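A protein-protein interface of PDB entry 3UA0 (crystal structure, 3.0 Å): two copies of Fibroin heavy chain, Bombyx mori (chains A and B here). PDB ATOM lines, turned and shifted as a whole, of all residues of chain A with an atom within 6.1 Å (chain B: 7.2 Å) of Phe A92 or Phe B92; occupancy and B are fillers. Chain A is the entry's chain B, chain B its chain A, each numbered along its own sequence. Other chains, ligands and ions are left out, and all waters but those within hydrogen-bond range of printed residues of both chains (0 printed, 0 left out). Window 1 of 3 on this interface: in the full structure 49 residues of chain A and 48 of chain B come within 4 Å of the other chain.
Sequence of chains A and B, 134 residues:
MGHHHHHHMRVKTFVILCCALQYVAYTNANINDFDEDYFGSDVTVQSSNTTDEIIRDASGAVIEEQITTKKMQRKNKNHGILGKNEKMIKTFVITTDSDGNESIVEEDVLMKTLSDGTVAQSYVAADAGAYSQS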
ATOM      1  N   PHE A  34     -20.684  -8.707 -12.117  1.00  0.00           N
ATOM      2  CA  PHE A  34     -21.900  -7.925 -12.312  1.00  0.00           C
ATOM      3  C   PHE A  34     -22.551  -8.179 -13.665  1.00  0.00           C
ATOM      4  O   PHE A  34     -23.666  -7.724 -13.930  1.00  0.00           O
ATOM      5  CB  PHE A  34     -21.592  -6.433 -12.151  1.00  0.00           C
ATOM      6  CG  PHE A  34     -21.340  -6.018 -10.729  1.00  0.00           C
ATOM      7  CD1 PHE A  34     -22.377  -5.521  -9.944  1.00  0.00           C
ATOM      8  CD2 PHE A  34     -20.071  -6.130 -10.170  1.00  0.00           C
ATOM      9  CE1 PHE A  34     -22.158  -5.146  -8.632  1.00  0.00           C
ATOM     10  CE2 PHE A  34     -19.835  -5.753  -8.855  1.00  0.00           C
ATOM     11  CZ  PHE A  34     -20.880  -5.261  -8.085  1.00  0.00           C
ATOM     12  N   ASP A  35     -21.854  -8.913 -14.520  1.00  0.00           N
ATOM     13  CA  ASP A  35     -22.388  -9.251 -15.828  1.00  0.00           C
ATOM     14  C   ASP A  35     -22.909 -10.694 -15.817  1.00  0.00           C
ATOM     15  O   ASP A  35     -22.738 -11.435 -16.782  1.00  0.00           O
ATOM     16  CB  ASP A  35     -21.313  -9.025 -16.898  1.00  0.00           C
ATOM     17  CG  ASP A  35     -20.651  -7.642 -16.783  1.00  0.00           C
ATOM     18  OD1 ASP A  35     -21.387  -6.650 -16.570  1.00  0.00           O
ATOM     19  OD2 ASP A  35     -19.405  -7.547 -16.905  1.00  0.00           O
ATOM     20  N   LYS A  71     -33.135  -9.163  -5.601  1.00  0.00           N
ATOM     21  CA  LYS A  71     -32.541 -10.341  -4.994  1.00  0.00           C
ATOM     22  C   LYS A  71     -32.160 -10.086  -3.541  1.00  0.00           C
ATOM     23  O   LYS A  71     -32.552  -9.078  -2.950  1.00  0.00           O
ATOM     24  CB  LYS A  71     -31.319 -10.795  -5.786  1.00  0.00           C
ATOM     25  CG  LYS A  71     -31.631 -11.183  -7.204  1.00  0.00           C
ATOM     26  CD  LYS A  71     -30.396 -11.718  -7.887  1.00  0.00           C
ATOM     27  CE  LYS A  71     -29.470 -10.590  -8.247  1.00  0.00           C
ATOM     28  NZ  LYS A  71     -30.203  -9.534  -8.989  1.00  0.00           N
ATOM     29  N   LYS A  90     -23.982   0.540  -1.722  1.00  0.00           N
ATOM     30  CA  LYS A  90     -23.242   0.715  -2.970  1.00  0.00           C
ATOM     31  C   LYS A  90     -24.165   0.762  -4.199  1.00  0.00           C
ATOM     32  O   LYS A  90     -25.156   0.050  -4.293  1.00  0.00           O
ATOM     33  CB  LYS A  90     -22.205  -0.397  -3.146  1.00  0.00           C
ATOM     34  CG  LYS A  90     -21.580  -0.850  -1.860  1.00  0.00           C
ATOM     35  CD  LYS A  90     -20.610  -1.988  -2.101  1.00  0.00           C
ATOM     36  CE  LYS A  90     -19.301  -1.508  -2.724  1.00  0.00           C
ATOM     37  NZ  LYS A  90     -18.346  -2.642  -2.978  1.00  0.00           N
ATOM     38  N   THR A  91     -23.810   1.605  -5.152  1.00  0.00           N
ATOM     39  CA  THR A  91     -24.585   1.754  -6.361  1.00  0.00           C
ATOM     40  C   THR A  91     -23.705   1.545  -7.573  1.00  0.00           C
ATOM     41  O   THR A  91     -22.548   1.953  -7.596  1.00  0.00           O
ATOM     42  CB  THR A  91     -25.169   3.146  -6.435  1.00  0.00           C
ATOM     43  OG1 THR A  91     -26.580   3.068  -6.210  1.00  0.00           O
ATOM     44  CG2 THR A  91     -24.872   3.782  -7.807  1.00  0.00           C
ATOM     45  N   PHE A  92     -24.255   0.898  -8.587  1.00  0.00           N
ATOM     46  CA  PHE A  92     -23.498   0.654  -9.795  1.00  0.00           C
ATOM     47  C   PHE A  92     -24.363   0.958 -10.997  1.00  0.00           C
ATOM     48  O   PHE A  92     -25.552   0.678 -10.998  1.00  0.00           O
ATOM     49  CB  PHE A  92     -23.018  -0.795  -9.861  1.00  0.00           C
ATOM     50  CG  PHE A  92     -21.927  -1.127  -8.890  1.00  0.00           C
ATOM     51  CD1 PHE A  92     -20.603  -1.153  -9.299  1.00  0.00           C
ATOM     52  CD2 PHE A  92     -22.222  -1.443  -7.573  1.00  0.00           C
ATOM     53  CE1 PHE A  92     -19.584  -1.479  -8.405  1.00  0.00           C
ATOM     54  CE2 PHE A  92     -21.209  -1.765  -6.673  1.00  0.00           C
ATOM     55  CZ  PHE A  92     -19.891  -1.783  -7.093  1.00  0.00           C
ATOM     56  N   VAL A  93     -23.750   1.547 -12.014  1.00  0.00           N
ATOM     57  CA  VAL A  93     -24.422   1.797 -13.268  1.00  0.00           C
ATOM     58  C   VAL A  93     -23.457   1.446 -14.398  1.00  0.00           C
ATOM     59  O   VAL A  93     -22.541   2.210 -14.722  1.00  0.00           O
ATOM     60  CB  VAL A  93     -24.956   3.257 -13.375  1.00  0.00           C
ATOM     61  CG1 VAL A  93     -25.586   3.510 -14.736  1.00  0.00           C
ATOM     62  CG2 VAL A  93     -25.969   3.543 -12.271  1.00  0.00           C
ATOM     63  N   ILE A  94     -23.677   0.270 -14.984  1.00  0.00           N
ATOM     64  CA  ILE A  94     -22.823  -0.249 -16.043  1.00  0.00           C
ATOM     65  C   ILE A  94     -23.454  -0.077 -17.416  1.00  0.00           C
ATOM     66  O   ILE A  94     -24.462  -0.700 -17.735  1.00  0.00           O
ATOM     67  CB  ILE A  94     -22.504  -1.742 -15.854  1.00  0.00           C
ATOM     68  CG1 ILE A  94     -21.839  -2.000 -14.502  1.00  0.00           C
ATOM     69  CG2 ILE A  94     -21.605  -2.226 -16.970  1.00  0.00           C
ATOM     70  CD1 ILE A  94     -22.777  -1.961 -13.317  1.00  0.00           C
ATOM     71  N   ILE A 104     -18.433   1.776 -16.070  1.00  0.00           N
ATOM     72  CA  ILE A 104     -19.062   1.660 -14.768  1.00  0.00           C
ATOM     73  C   ILE A 104     -18.981   2.993 -14.029  1.00  0.00           C
ATOM     74  O   ILE A 104     -18.110   3.817 -14.280  1.00  0.00           O
ATOM     75  CB  ILE A 104     -18.354   0.584 -13.900  1.00  0.00           C
ATOM     76  CG1 ILE A 104     -18.116  -0.695 -14.698  1.00  0.00           C
ATOM     77  CG2 ILE A 104     -19.133   0.293 -12.613  1.00  0.00           C
ATOM     78  CD1 ILE A 104     -16.976  -0.608 -15.690  1.00  0.00           C
ATOM     79  N   VAL A 105     -19.919   3.190 -13.116  1.00  0.00           N
ATOM     80  CA  VAL A 105     -19.906   4.316 -12.207  1.00  0.00           C
ATOM     81  C   VAL A 105     -20.414   3.779 -10.878  1.00  0.00           C
ATOM     82  O   VAL A 105     -21.579   3.394 -10.748  1.00  0.00           O
ATOM     83  CB  VAL A 105     -20.804   5.462 -12.703  1.00  0.00           C
ATOM     84  CG1 VAL A 105     -21.241   6.343 -11.551  1.00  0.00           C
ATOM     85  CG2 VAL A 105     -20.087   6.270 -13.762  1.00  0.00           C
ATOM     86  N   GLU A 106     -19.516   3.718  -9.903  1.00  0.00           N
ATOM     87  CA  GLU A 106     -19.874   3.255  -8.581  1.00  0.00           C
ATOM     88  C   GLU A 106     -20.094   4.444  -7.666  1.00  0.00           C
ATOM     89  O   GLU A 106     -19.552   5.514  -7.885  1.00  0.00           O
ATOM     90  CB  GLU A 106     -18.786   2.347  -8.019  1.00  0.00           C
ATOM     91  CG  GLU A 106     -19.196   1.619  -6.759  1.00  0.00           C
ATOM     92  CD  GLU A 106     -18.093   0.743  -6.230  1.00  0.00           C
ATOM     93  OE1 GLU A 106     -17.131   0.486  -6.991  1.00  0.00           O
ATOM     94  OE2 GLU A 106     -18.184   0.314  -5.060  1.00  0.00           O
ATOM     95  N   GLU A 107     -20.944   4.260  -6.669  1.00  0.00           N
ATOM     96  CA  GLU A 107     -21.091   5.230  -5.609  1.00  0.00           C
ATOM     97  C   GLU A 107     -21.356   4.495  -4.310  1.00  0.00           C
ATOM     98  O   GLU A 107     -22.380   3.835  -4.145  1.00  0.00           O
ATOM     99  CB  GLU A 107     -22.196   6.231  -5.891  1.00  0.00           C
ATOM    100  CG  GLU A 107     -22.454   7.168  -4.716  1.00  0.00           C
ATOM    101  CD  GLU A 107     -23.065   8.500  -5.140  1.00  0.00           C
ATOM    102  OE1 GLU A 107     -22.454   9.191  -5.984  1.00  0.00           O
ATOM    103  OE2 GLU A 107     -24.147   8.865  -4.622  1.00  0.00           O
ATOM    104  N   ASP A 108     -20.392   4.600  -3.402  1.00  0.00           N
ATOM    105  CA  ASP A 108     -20.488   3.994  -2.098  1.00  0.00           C
ATOM    106  C   ASP A 108     -20.959   5.051  -1.120  1.00  0.00           C
ATOM    107  O   ASP A 108     -20.339   6.107  -0.987  1.00  0.00           O
ATOM    108  CB  ASP A 108     -19.127   3.452  -1.676  1.00  0.00           C
ATOM    109  CG  ASP A 108     -18.520   2.524  -2.713  1.00  0.00           C
ATOM    110  OD1 ASP A 108     -19.285   1.908  -3.485  1.00  0.00           O
ATOM    111  OD2 ASP A 108     -17.278   2.402  -2.759  1.00  0.00           O
ATOM    112  N   LYS B  70     -16.682   6.683  -7.838  1.00  0.00           N
ATOM    113  CA  LYS B  70     -15.688   6.264  -8.817  1.00  0.00           C
ATOM    114  C   LYS B  70     -16.278   6.186 -10.232  1.00  0.00           C
ATOM    115  O   LYS B  70     -17.440   5.831 -10.424  1.00  0.00           O
ATOM    116  CB  LYS B  70     -15.085   4.905  -8.435  1.00  0.00           C
ATOM    117  CG  LYS B  70     -15.100   4.570  -6.952  1.00  0.00           C
ATOM    118  CD  LYS B  70     -14.432   3.218  -6.691  1.00  0.00           C
ATOM    119  CE  LYS B  70     -14.699   2.692  -5.278  1.00  0.00           C
ATOM    120  NZ  LYS B  70     -14.198   1.286  -5.094  1.00  0.00           N
ATOM    121  N   MET B  72     -15.035   4.283 -13.694  1.00  0.00           N
ATOM    122  CA  MET B  72     -14.082   3.316 -14.214  1.00  0.00           C
ATOM    123  C   MET B  72     -14.540   2.925 -15.600  1.00  0.00           C
ATOM    124  O   MET B  72     -15.721   2.949 -15.872  1.00  0.00           O
ATOM    125  CB  MET B  72     -14.048   2.093 -13.304  1.00  0.00           C
ATOM    126  CG  MET B  72     -14.103   2.462 -11.828  1.00  0.00           C
ATOM    127  SD  MET B  72     -15.016   1.157 -10.684  1.00  0.00           S
ATOM    128  CE  MET B  72     -13.488   0.073 -10.146  1.00  0.00           C
ATOM    129  N   ILE B  89     -27.694  -1.224 -20.063  1.00  0.00           N
ATOM    130  CA  ILE B  89     -27.608  -0.357 -18.919  1.00  0.00           C
ATOM    131  C   ILE B  89     -28.182  -1.081 -17.702  1.00  0.00           C
ATOM    132  O   ILE B  89     -29.370  -0.988 -17.378  1.00  0.00           O
ATOM    133  CB  ILE B  89     -28.313   1.000 -19.168  1.00  0.00           C
ATOM    134  CG1 ILE B  89     -27.799   1.650 -20.451  1.00  0.00           C
ATOM    135  CG2 ILE B  89     -28.096   1.958 -18.003  1.00  0.00           C
ATOM    136  CD1 ILE B  89     -28.222   3.098 -20.597  1.00  0.00           C
ATOM    137  N   LYS B  90     -27.303  -1.814 -17.033  1.00  0.00           N
ATOM    138  CA  LYS B  90     -27.612  -2.397 -15.746  1.00  0.00           C
ATOM    139  C   LYS B  90     -27.377  -1.364 -14.631  1.00  0.00           C
ATOM    140  O   LYS B  90     -26.411  -0.603 -14.665  1.00  0.00           O
ATOM    141  CB  LYS B  90     -26.753  -3.641 -15.546  1.00  0.00           C
ATOM    142  CG  LYS B  90     -26.532  -4.410 -16.848  1.00  0.00           C
ATOM    143  CD  LYS B  90     -25.457  -5.490 -16.725  1.00  0.00           C
ATOM    144  CE  LYS B  90     -24.657  -5.635 -18.025  1.00  0.00           C
ATOM    145  NZ  LYS B  90     -23.763  -4.453 -18.300  1.00  0.00           N
ATOM    146  N   THR B  91     -28.307  -1.324 -13.681  1.00  0.00           N
ATOM    147  CA  THR B  91     -28.218  -0.490 -12.491  1.00  0.00           C
ATOM    148  C   THR B  91     -28.311  -1.389 -11.267  1.00  0.00           C
ATOM    149  O   THR B  91     -29.214  -2.209 -11.159  1.00  0.00           O
ATOM    150  CB  THR B  91     -29.393   0.493 -12.393  1.00  0.00           C
ATOM    151  OG1 THR B  91     -29.197   1.586 -13.290  1.00  0.00           O
ATOM    152  CG2 THR B  91     -29.516   1.037 -10.984  1.00  0.00           C
ATOM    153  N   PHE B  92     -27.382  -1.235 -10.335  1.00  0.00           N
ATOM    154  CA  PHE B  92     -27.416  -2.029  -9.121  1.00  0.00           C
ATOM    155  C   PHE B  92     -27.559  -1.151  -7.903  1.00  0.00           C
ATOM    156  O   PHE B  92     -27.187   0.017  -7.929  1.00  0.00           O
ATOM    157  CB  PHE B  92     -26.176  -2.895  -9.030  1.00  0.00           C
ATOM    158  CG  PHE B  92     -26.094  -3.910 -10.121  1.00  0.00           C
ATOM    159  CD1 PHE B  92     -26.583  -5.193  -9.928  1.00  0.00           C
ATOM    160  CD2 PHE B  92     -25.566  -3.576 -11.357  1.00  0.00           C
ATOM    161  CE1 PHE B  92     -26.519  -6.135 -10.935  1.00  0.00           C
ATOM    162  CE2 PHE B  92     -25.501  -4.516 -12.377  1.00  0.00           C
ATOM    163  CZ  PHE B  92     -25.978  -5.798 -12.163  1.00  0.00           C
ATOM    164  N   VAL B  93     -28.125  -1.710  -6.845  1.00  0.00           N
ATOM    165  CA  VAL B  93     -28.397  -0.946  -5.641  1.00  0.00           C
ATOM    166  C   VAL B  93     -28.363  -1.882  -4.450  1.00  0.00           C
ATOM    167  O   VAL B  93     -29.395  -2.324  -3.945  1.00  0.00           O
ATOM    168  CB  VAL B  93     -29.748  -0.213  -5.717  1.00  0.00           C
ATOM    169  CG1 VAL B  93     -30.119   0.387  -4.368  1.00  0.00           C
ATOM    170  CG2 VAL B  93     -29.708   0.865  -6.785  1.00  0.00           C
ATOM    171  N   ILE B  94     -27.152  -2.179  -4.006  1.00  0.00           N
ATOM    172  CA  ILE B  94     -26.942  -3.151  -2.958  1.00  0.00           C
ATOM    173  C   ILE B  94     -26.912  -2.481  -1.598  1.00  0.00           C
ATOM    174  O   ILE B  94     -26.323  -1.421  -1.438  1.00  0.00           O
ATOM    175  CB  ILE B  94     -25.640  -3.895  -3.195  1.00  0.00           C
ATOM    176  CG1 ILE B  94     -25.492  -4.189  -4.690  1.00  0.00           C
ATOM    177  CG2 ILE B  94     -25.615  -5.170  -2.377  1.00  0.00           C
ATOM    178  CD1 ILE B  94     -24.083  -4.450  -5.129  1.00  0.00           C
ATOM    179  N   ILE B 104     -29.897  -6.831  -3.081  1.00  0.00           N
ATOM    180  CA  ILE B 104     -29.644  -6.371  -4.441  1.00  0.00           C
ATOM    181  C   ILE B 104     -30.902  -5.998  -5.226  1.00  0.00           C
ATOM    182  O   ILE B 104     -31.864  -6.763  -5.297  1.00  0.00           O
ATOM    183  CB  ILE B 104     -28.914  -7.455  -5.236  1.00  0.00           C
ATOM    184  CG1 ILE B 104     -27.747  -7.992  -4.409  1.00  0.00           C
ATOM    185  CG2 ILE B 104     -28.476  -6.918  -6.599  1.00  0.00           C
ATOM    186  CD1 ILE B 104     -27.722  -9.493  -4.327  1.00  0.00           C
ATOM    187  N   VAL B 105     -30.870  -4.813  -5.820  1.00  0.00           N
ATOM    188  CA  VAL B 105     -31.876  -4.400  -6.782  1.00  0.00           C
ATOM    189  C   VAL B 105     -31.197  -4.264  -8.144  1.00  0.00           C
ATOM    190  O   VAL B 105     -30.174  -3.595  -8.268  1.00  0.00           O
ATOM    191  CB  VAL B 105     -32.516  -3.061  -6.378  1.00  0.00           C
ATOM    192  CG1 VAL B 105     -33.438  -2.567  -7.458  1.00  0.00           C
ATOM    193  CG2 VAL B 105     -33.267  -3.218  -5.080  1.00  0.00           C
ATOM    194  N   GLU B 106     -31.743  -4.921  -9.160  1.00  0.00           N
ATOM    195  CA  GLU B 106     -31.151  -4.858 -10.488  1.00  0.00           C
ATOM    196  C   GLU B 106     -32.114  -4.258 -11.507  1.00  0.00           C
ATOM    197  O   GLU B 106     -33.304  -4.540 -11.481  1.00  0.00           O
ATOM    198  CB  GLU B 106     -30.697  -6.243 -10.948  1.00  0.00           C
ATOM    199  CG  GLU B 106     -29.941  -6.202 -12.265  1.00  0.00           C
ATOM    200  CD  GLU B 106     -29.200  -7.492 -12.570  1.00  0.00           C
ATOM    201  OE1 GLU B 106     -29.269  -8.437 -11.748  1.00  0.00           O
ATOM    202  OE2 GLU B 106     -28.545  -7.553 -13.638  1.00  0.00           O
ATOM    203  N   GLU B 107     -31.599  -3.415 -12.397  1.00  0.00           N
ATOM    204  CA  GLU B 107     -32.398  -2.911 -13.504  1.00  0.00           C
ATOM    205  C   GLU B 107     -31.622  -2.961 -14.809  1.00  0.00           C
ATOM    206  O   GLU B 107     -30.613  -2.268 -14.983  1.00  0.00           O
ATOM    207  CB  GLU B 107     -32.911  -1.499 -13.246  1.00  0.00           C
ATOM    208  CG  GLU B 107     -33.174  -0.744 -14.537  1.00  0.00           C
ATOM    209  CD  GLU B 107     -34.404   0.144 -14.484  1.00  0.00           C
ATOM    210  OE1 GLU B 107     -35.227  -0.033 -13.563  1.00  0.00           O
ATOM    211  OE2 GLU B 107     -34.555   1.016 -15.373  1.00  0.00           O
ATOM    212  N   ASP B 108     -32.101  -3.791 -15.724  1.00  0.00           N
ATOM    213  CA  ASP B 108     -31.496  -3.905 -17.037  1.00  0.00           C
ATOM    214  C   ASP B 108     -32.339  -3.167 -18.049  1.00  0.00           C
ATOM    215  O   ASP B 108     -33.559  -3.281 -18.054  1.00  0.00           O
ATOM    216  CB  ASP B 108     -31.368  -5.363 -17.432  1.00  0.00           C
ATOM    217  CG  ASP B 108     -30.849  -6.210 -16.306  1.00  0.00           C
ATOM    218  OD1 ASP B 108     -29.627  -6.146 -16.030  1.00  0.00           O
ATOM    219  OD2 ASP B 108     -31.672  -6.931 -15.692  1.00  0.00           O
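Phe A92 touches just these residues of chain B: Lys B90 (3.98 Å), Thr B91 (3.3 Å) and Phe B92 (2.7 Å). Of chain A, only Phe A34, Thr A91, Phe A92 and Ile A94 come within 4 Å of Phe B92. Of the printed residues of chain B, Ile A104 touches Met B72. Printed residues of chain A within 4 Å of Ile B94: Lys A90. Of the printed residues of chain A, Lys B70 touches Val A105, Glu A106 and Asp A108. Of the printed residues of chain B, Ile A94 touches Ile B89 (3.4 Å), Lys B90 (2.9 Å) and Phe B92 (3.8 Å). Glu A107 touches none of the printed residues of chain B. Val B105 touches none of the printed residues of chain A. The nearest residue of chain B that does not touch Phe A92 is Ile B94 (4.2 Å). The nearest residue of chain A that does not touch Phe B92 is Lys A90 (4.2 Å).
N of Thr B91 lies within hydrogen-bond range of O of Glu B107, 2.8 Å away. N of Val B93 sits at hydrogen-bond distance from O of Val B105, at 3.1 Å. The side-chain carboxylate (OE2) of Glu A106 lies within salt-bridge range of the side-chain amino group (NZ) of Lys A90 (3.6 Å). The backbone NH of Thr A91 is in hydrogen-bond range of the backbone carbonyl oxygen of Glu A107 (2.8 Å). The backbone NH (N) of Val A93 lies within hydrogen-bond range of the backbone carbonyl oxygen (O) of Val A105 (3.1 Å). OE2 of Glu A106 lies close to OD1 of Asp A108, at 2.5 Å.
NZ of Lys B70 lies within salt-bridge range of OE1 of Glu A106. N of Ile A104 is in hydrogen-bond range of O of Met B72 (3.0 Å). The side-chain carboxylate (OD1) of Asp A35 lies within salt-bridge range of the side-chain amino group (NZ) of Lys B90, 3.7 Å away. The backbone NH of Ile A94 sits at hydrogen-bond distance from the backbone carbonyl oxygen of Lys B90 (2.9 Å). N of Phe B92 lies within hydrogen-bond range of O of Phe A92 (2.7 Å). N of Ile B94 sits at hydrogen-bond distance from O of Lys A90. N of Lys A71 sits at hydrogen-bond distance from O of Ile B104, 2.7 Å away. OE1 of Glu B106 lies within salt-bridge range of NZ of Lys A71, 3.1 Å away.
Lys A90 touches Val B93, and with the chains exchanged Val A93 touches Lys B90. Lys A90 touches Ile B94, and with the chains exchanged Ile A94 touches Lys B90. Phe A92 touches Lys B90, but with the chains exchanged Lys A90 does not touch Phe B92 (4.2 Å). Ile A94 touches Phe B92, but with the chains exchanged Phe A92 does not touch Ile B94 (4.2 Å). Of the 20 pairs that touch across the chains among the printed residues, 9 have their exchanged pair printed and touching as well.
Printed residues of chain A that touch a printed residue of chain B: Phe A34, Asp A35, Lys A71, Lys A90, Thr A91, Phe A92, Val A93, Ile A94, Ile A104, Val A105, Glu A106 and Asp A108. Hydrophobic or aromatic side chains of chain A that line the printed part of chain B: Phe A34, Phe A92, Val A93, Ile A94, Ile A104 and Val A105. Printed residues of chain B that touch a printed residue of chain A: Lys B70, Met B72, Ile B89, Lys B90, Thr B91, Phe B92, Val B93, Ile B94, Ile B104 and Glu B106. Hydrophobic or aromatic side chains of chain B that line the printed part of chain A: Phe B92, Val B93 and Ile B104. Among the printed residues, 20 pairs touch across the chains.
CA of Val B93 touches O of Lys A90 (3.6 Å). CA of Thr A91 touches O of Phe B92, at 3.5 Å. Thr A91 touches Val B93. O of Phe A92 touches CA of Thr B91 (3.3 Å). Val A93 touches Lys B90. Thr B91 touches Val A93 (OG1 to CG2, 3.9 Å). CA of Ile B89 touches O of Ile A94, at 3.4 Å. CD1 of Ile A94 touches CD2 of Phe B92, at 3.8 Å. Val A105 touches Lys B70. Asp A108 touches Lys B70 (OD2 to CE, 3.6 Å).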
